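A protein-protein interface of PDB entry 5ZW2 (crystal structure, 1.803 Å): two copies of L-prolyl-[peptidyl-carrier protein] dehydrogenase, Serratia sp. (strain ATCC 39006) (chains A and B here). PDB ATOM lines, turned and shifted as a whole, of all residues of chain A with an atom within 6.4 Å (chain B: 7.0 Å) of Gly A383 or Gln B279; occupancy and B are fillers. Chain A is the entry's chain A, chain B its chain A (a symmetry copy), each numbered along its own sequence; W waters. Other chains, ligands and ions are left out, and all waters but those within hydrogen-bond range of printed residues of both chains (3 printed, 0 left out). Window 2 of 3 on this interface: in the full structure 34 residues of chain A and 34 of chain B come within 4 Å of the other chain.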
ATOM      1  N   GLU A 373      -3.438 -23.624   4.482  1.00  0.00           N
ATOM      2  CA  GLU A 373      -3.077 -23.584   5.902  1.00  0.00           C
ATOM      3  C   GLU A 373      -2.816 -22.157   6.361  1.00  0.00           C
ATOM      4  O   GLU A 373      -3.087 -21.803   7.514  1.00  0.00           O
ATOM      5  CB  GLU A 373      -1.807 -24.418   6.169  1.00  0.00           C
ATOM      6  CG  GLU A 373      -2.061 -25.942   6.019  1.00  0.00           C
ATOM      7  CD  GLU A 373      -3.179 -26.392   6.968  1.00  0.00           C
ATOM      8  OE1 GLU A 373      -2.938 -26.394   8.151  1.00  0.00           O
ATOM      9  OE2 GLU A 373      -4.263 -26.608   6.474  1.00  0.00           O
ATOM     10  N   ARG A 377      -4.978 -20.191   9.165  1.00  0.00           N
ATOM     11  CA  ARG A 377      -4.395 -19.561  10.343  1.00  0.00           C
ATOM     12  C   ARG A 377      -4.852 -18.113  10.480  1.00  0.00           C
ATOM     13  O   ARG A 377      -5.227 -17.661  11.595  1.00  0.00           O
ATOM     14  CB  ARG A 377      -2.861 -19.670  10.291  1.00  0.00           C
ATOM     15  CG  ARG A 377      -2.093 -18.929  11.455  1.00  0.00           C
ATOM     16  CD  ARG A 377      -0.645 -19.368  11.421  1.00  0.00           C
ATOM     17  NE  ARG A 377       0.040 -19.105  10.132  1.00  0.00           N
ATOM     18  CZ  ARG A 377       0.331 -17.881   9.647  1.00  0.00           C
ATOM     19  NH1 ARG A 377      -0.006 -16.773  10.326  1.00  0.00           N
ATOM     20  NH2 ARG A 377       0.971 -17.750   8.483  1.00  0.00           N
ATOM     21  N   GLY A 380      -8.232 -17.713  11.898  1.00  0.00           N
ATOM     22  CA  GLY A 380      -8.392 -18.100  13.283  1.00  0.00           C
ATOM     23  C   GLY A 380      -8.710 -19.558  13.503  1.00  0.00           C
ATOM     24  O   GLY A 380      -9.225 -19.894  14.582  1.00  0.00           O
ATOM     25  N   LEU A 381      -8.431 -20.440  12.511  1.00  0.00           N
ATOM     26  CA  LEU A 381      -8.778 -21.870  12.547  1.00  0.00           C
ATOM     27  C   LEU A 381      -7.609 -22.708  12.979  1.00  0.00           C
ATOM     28  O   LEU A 381      -7.668 -23.942  12.928  1.00  0.00           O
ATOM     29  CB  LEU A 381      -9.292 -22.334  11.165  1.00  0.00           C
ATOM     30  CG  LEU A 381     -10.537 -21.573  10.696  1.00  0.00           C
ATOM     31  CD1 LEU A 381     -10.973 -22.055   9.308  1.00  0.00           C
ATOM     32  CD2 LEU A 381     -11.767 -21.658  11.686  1.00  0.00           C
ATOM     33  N   ARG A 382      -6.510 -22.068  13.377  1.00  0.00           N
ATOM     34  CA  ARG A 382      -5.341 -22.816  13.787  1.00  0.00           C
ATOM     35  C   ARG A 382      -4.926 -22.341  15.185  1.00  0.00           C
ATOM     36  O   ARG A 382      -3.741 -22.266  15.496  1.00  0.00           O
ATOM     37  CB  ARG A 382      -4.209 -22.677  12.789  1.00  0.00           C
ATOM     38  CG  ARG A 382      -4.532 -23.190  11.347  1.00  0.00           C
ATOM     39  CD  ARG A 382      -4.485 -24.732  11.335  1.00  0.00           C
ATOM     40  NE  ARG A 382      -4.840 -25.325  10.044  1.00  0.00           N
ATOM     41  CZ  ARG A 382      -6.081 -25.679   9.721  1.00  0.00           C
ATOM     42  NH1 ARG A 382      -6.315 -26.303   8.545  1.00  0.00           N
ATOM     43  NH2 ARG A 382      -7.101 -25.352  10.542  1.00  0.00           N
ATOM     44  N   GLY A 383      -5.913 -22.051  16.023  1.00  0.00           N
ATOM     45  CA  GLY A 383      -5.702 -21.491  17.360  1.00  0.00           C
ATOM     46  C   GLY A 383      -5.351 -22.583  18.330  1.00  0.00           C
ATOM     47  O   GLY A 383      -4.733 -23.560  17.892  1.00  0.00           O
ATOM     48  N   ALA B 267     -17.004 -23.131  13.675  1.00  0.00           N
ATOM     49  CA  ALA B 267     -15.862 -24.016  13.458  1.00  0.00           C
ATOM     50  C   ALA B 267     -14.764 -23.801  14.478  1.00  0.00           C
ATOM     51  O   ALA B 267     -13.979 -24.721  14.733  1.00  0.00           O
ATOM     52  CB  ALA B 267     -15.278 -23.842  12.033  1.00  0.00           C
ATOM     53  N   LYS B 275     -10.300 -31.168  19.678  1.00  0.00           N
ATOM     54  CA  LYS B 275      -9.920 -29.885  19.097  1.00  0.00           C
ATOM     55  C   LYS B 275     -11.098 -29.265  18.376  1.00  0.00           C
ATOM     56  O   LYS B 275     -12.081 -29.941  18.080  1.00  0.00           O
ATOM     57  CB  LYS B 275      -8.760 -30.090  18.132  1.00  0.00           C
ATOM     58  CG  LYS B 275      -9.174 -30.990  16.943  1.00  0.00           C
ATOM     59  CD  LYS B 275      -7.910 -31.465  16.156  1.00  0.00           C
ATOM     60  CE  LYS B 275      -7.265 -32.647  16.940  1.00  0.00           C
ATOM     61  NZ  LYS B 275      -5.912 -32.949  16.452  1.00  0.00           N
ATOM     62  N   ALA B 276     -10.950 -27.987  18.005  1.00  0.00           N
ATOM     63  CA  ALA B 276     -12.000 -27.328  17.215  1.00  0.00           C
ATOM     64  C   ALA B 276     -12.132 -28.005  15.849  1.00  0.00           C
ATOM     65  O   ALA B 276     -11.133 -28.386  15.237  1.00  0.00           O
ATOM     66  CB  ALA B 276     -11.666 -25.866  17.033  1.00  0.00           C
ATOM     67  N   ILE B 277     -13.380 -28.165  15.345  1.00  0.00           N
ATOM     68  CA  ILE B 277     -13.498 -28.903  14.074  1.00  0.00           C
ATOM     69  C   ILE B 277     -12.804 -28.130  12.934  1.00  0.00           C
ATOM     70  O   ILE B 277     -12.424 -28.740  11.939  1.00  0.00           O
ATOM     71  CB  ILE B 277     -14.969 -29.177  13.656  1.00  0.00           C
ATOM     72  CG1 ILE B 277     -15.779 -27.893  13.695  1.00  0.00           C
ATOM     73  CG2 ILE B 277     -15.555 -30.221  14.653  1.00  0.00           C
ATOM     74  CD1 ILE B 277     -17.324 -28.034  13.128  1.00  0.00           C
ATOM     75  N   GLY B 278     -12.665 -26.818  13.051  1.00  0.00           N
ATOM     76  CA  GLY B 278     -11.932 -26.036  12.042  1.00  0.00           C
ATOM     77  C   GLY B 278     -10.469 -26.454  11.879  1.00  0.00           C
ATOM     78  O   GLY B 278      -9.842 -26.056  10.881  1.00  0.00           O
ATOM     79  N   GLN B 279      -9.913 -27.244  12.808  1.00  0.00           N
ATOM     80  CA  GLN B 279      -8.519 -27.694  12.739  1.00  0.00           C
ATOM     81  C   GLN B 279      -8.341 -28.835  11.764  1.00  0.00           C
ATOM     82  O   GLN B 279      -7.215 -29.096  11.359  1.00  0.00           O
ATOM     83  CB  GLN B 279      -7.988 -28.145  14.114  1.00  0.00           C
ATOM     84  CG  GLN B 279      -8.061 -27.025  15.153  1.00  0.00           C
ATOM     85  CD  GLN B 279      -6.732 -26.416  15.428  1.00  0.00           C
ATOM     86  OE1 GLN B 279      -5.785 -26.558  14.638  1.00  0.00           O
ATOM     87  NE2 GLN B 279      -6.630 -25.745  16.540  1.00  0.00           N
ATOM     88  N   PHE B 280      -9.426 -29.506  11.356  1.00  0.00           N
ATOM     89  CA  PHE B 280      -9.358 -30.596  10.371  1.00  0.00           C
ATOM     90  C   PHE B 280      -9.425 -29.997   8.976  1.00  0.00           C
ATOM     91  O   PHE B 280     -10.280 -29.157   8.724  1.00  0.00           O
ATOM     92  CB  PHE B 280     -10.556 -31.542  10.532  1.00  0.00           C
ATOM     93  CG  PHE B 280     -10.542 -32.236  11.827  1.00  0.00           C
ATOM     94  CD1 PHE B 280      -9.624 -33.233  12.053  1.00  0.00           C
ATOM     95  CD2 PHE B 280     -11.446 -31.888  12.789  1.00  0.00           C
ATOM     96  CE1 PHE B 280      -9.566 -33.847  13.331  1.00  0.00           C
ATOM     97  CE2 PHE B 280     -11.411 -32.480  14.066  1.00  0.00           C
ATOM     98  CZ  PHE B 280     -10.471 -33.436  14.331  1.00  0.00           C
ATOM     99  N   GLN B 281      -8.514 -30.413   8.087  1.00  0.00           N
ATOM    100  CA  GLN B 281      -8.463 -29.798   6.769  1.00  0.00           C
ATOM    101  C   GLN B 281      -9.739 -30.024   5.949  1.00  0.00           C
ATOM    102  O   GLN B 281     -10.092 -29.154   5.132  1.00  0.00           O
ATOM    103  CB  GLN B 281      -7.214 -30.290   6.004  1.00  0.00           C
ATOM    104  CG  GLN B 281      -5.944 -29.596   6.636  1.00  0.00           C
ATOM    105  CD  GLN B 281      -4.623 -30.125   6.097  1.00  0.00           C
ATOM    106  OE1 GLN B 281      -4.591 -30.992   5.246  1.00  0.00           O
ATOM    107  NE2 GLN B 281      -3.529 -29.678   6.693  1.00  0.00           N
ATOM    108  N   SER B 282     -10.452 -31.156   6.125  1.00  0.00           N
ATOM    109  CA  SER B 282     -11.708 -31.266   5.381  1.00  0.00           C
ATOM    110  C   SER B 282     -12.633 -30.111   5.717  1.00  0.00           C
ATOM    111  O   SER B 282     -13.394 -29.643   4.854  1.00  0.00           O
ATOM    112  CB  SER B 282     -12.439 -32.560   5.688  1.00  0.00           C
ATOM    113  OG  SER B 282     -11.698 -33.650   5.074  1.00  0.00           O
ATOM    114  N   VAL B 283     -12.635 -29.705   6.981  1.00  0.00           N
ATOM    115  CA  VAL B 283     -13.530 -28.634   7.431  1.00  0.00           C
ATOM    116  C   VAL B 283     -13.007 -27.266   6.977  1.00  0.00           C
ATOM    117  O   VAL B 283     -13.759 -26.473   6.421  1.00  0.00           O
ATOM    118  CB  VAL B 283     -13.708 -28.671   8.955  1.00  0.00           C
ATOM    119  CG1 VAL B 283     -14.470 -27.411   9.425  1.00  0.00           C
ATOM    120  CG2 VAL B 283     -14.436 -29.976   9.383  1.00  0.00           C
ATOM    121  N   SER B 284     -11.743 -26.967   7.265  1.00  0.00           N
ATOM    122  CA  SER B 284     -11.219 -25.652   6.923  1.00  0.00           C
ATOM    123  C   SER B 284     -11.111 -25.470   5.425  1.00  0.00           C
ATOM    124  O   SER B 284     -11.348 -24.374   4.947  1.00  0.00           O
ATOM    125  CB  SER B 284      -9.853 -25.425   7.576  1.00  0.00           C
ATOM    126  OG  SER B 284      -8.868 -26.392   7.159  1.00  0.00           O
HETATM  127  O   HOH W   1      -5.003 -27.699  12.356  1.00  0.00           O
HETATM  128  O   HOH W   2      -7.303 -25.938   5.142  1.00  0.00           O
HETATM  129  O   HOH W   3     -10.399 -24.250  14.258  1.00  0.00           O
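Printed residues of chain B within 4 Å of Gly A383: Gln B279.
Gln B279 touches just these residues of chain A: Leu A381 (3.6 Å), Arg A382 (3.5 Å) and Gly A383 (3.2 Å).
Of the printed residues of chain A, Gly B278 touches Leu A381 and Arg A382.
Printed residues of chain A within 4 Å of Ser B284: Leu A381 (3.95 Å) and Arg A382 (2.9 Å).
Printed residues of chain B within 4 Å of Arg A382: Gly B278, Gln B279, Gln B281 and Ser B284.
Lys B275 touches none of the printed residues of chain A.
Ala B276 touches none of the printed residues of chain A.
The nearest printed residue of chain B that does not touch Gly A383 is Ala B276 (7.0 Å).
The nearest printed residue of chain B that does not touch Arg A382 is Phe B280 (4.8 Å).
No position is printed for both chains.
Of the 9 pairs that touch across the chains among the printed residues, none has its exchanged pair printed and touching as well.
Leu A381 touches Gly B278 (O to O, 3.7 Å).
Leu A381 touches Gln B279 (O to CD, 3.6 Å).
Leu A381 touches Ser B284.
Arg A382 touches Gln B279 (NH2 to CA, 3.5 Å).
Gln B281 touches Arg A382 (CG to NH1, 3.8 Å).
OG of Ser B284 lies within hydrogen-bond range of NH1 of Arg A382 (2.9 Å).
O of Gly A383 is in hydrogen-bond range of NE2 of Gln B279, 3.2 Å away.
NH2 of Arg A382 is in hydrogen-bond range of O of Gly B278 (2.9 Å).
OE2 of Glu A373 sits at hydrogen-bond distance from NE2 of Gln B281 (3.2 Å).
The backbone NH of Gly B278 is in hydrogen-bond range of the backbone carbonyl oxygen of Ala B267 (3.0 Å).
The side-chain hydroxyl (OG) of Ser B284 is in hydrogen-bond range of the backbone carbonyl oxygen (O) of Phe B280 (3.5 Å).
The guanidinium group of Arg A382 lies within salt-bridge range of the side-chain carboxylate of Glu A373 (2.9 Å).
Water W2 lies within hydrogen-bond range of the side-chain hydroxyl (OG) of Ser B284 (2.6 Å) and the side-chain carboxylate (OE2) of Glu A373 (3.4 Å).
Water W1 lies within hydrogen-bond range of the side-chain amide oxygen (OE1) of Gln B279 (2.7 Å) and the guanidinium group (NE) of Arg A382 (3.3 Å).
Water W3 lies within hydrogen-bond range of O of Leu A381 (3.1 Å) and N of Gln B279 (3.4 Å).
Of the 6 printed residues of chain A, 4 touch a printed residue of chain B.
Printed residues of chain A that touch a printed residue of chain B: Glu A373, Leu A381, Arg A382 and Gly A383.
Hydrophobic or aromatic side chains of chain A within 4 Å of the printed part of chain B: Leu A381.
Of the 11 printed residues of chain B, 4 touch a printed residue of chain A.
Among the printed residues, 9 pairs touch across the chains.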
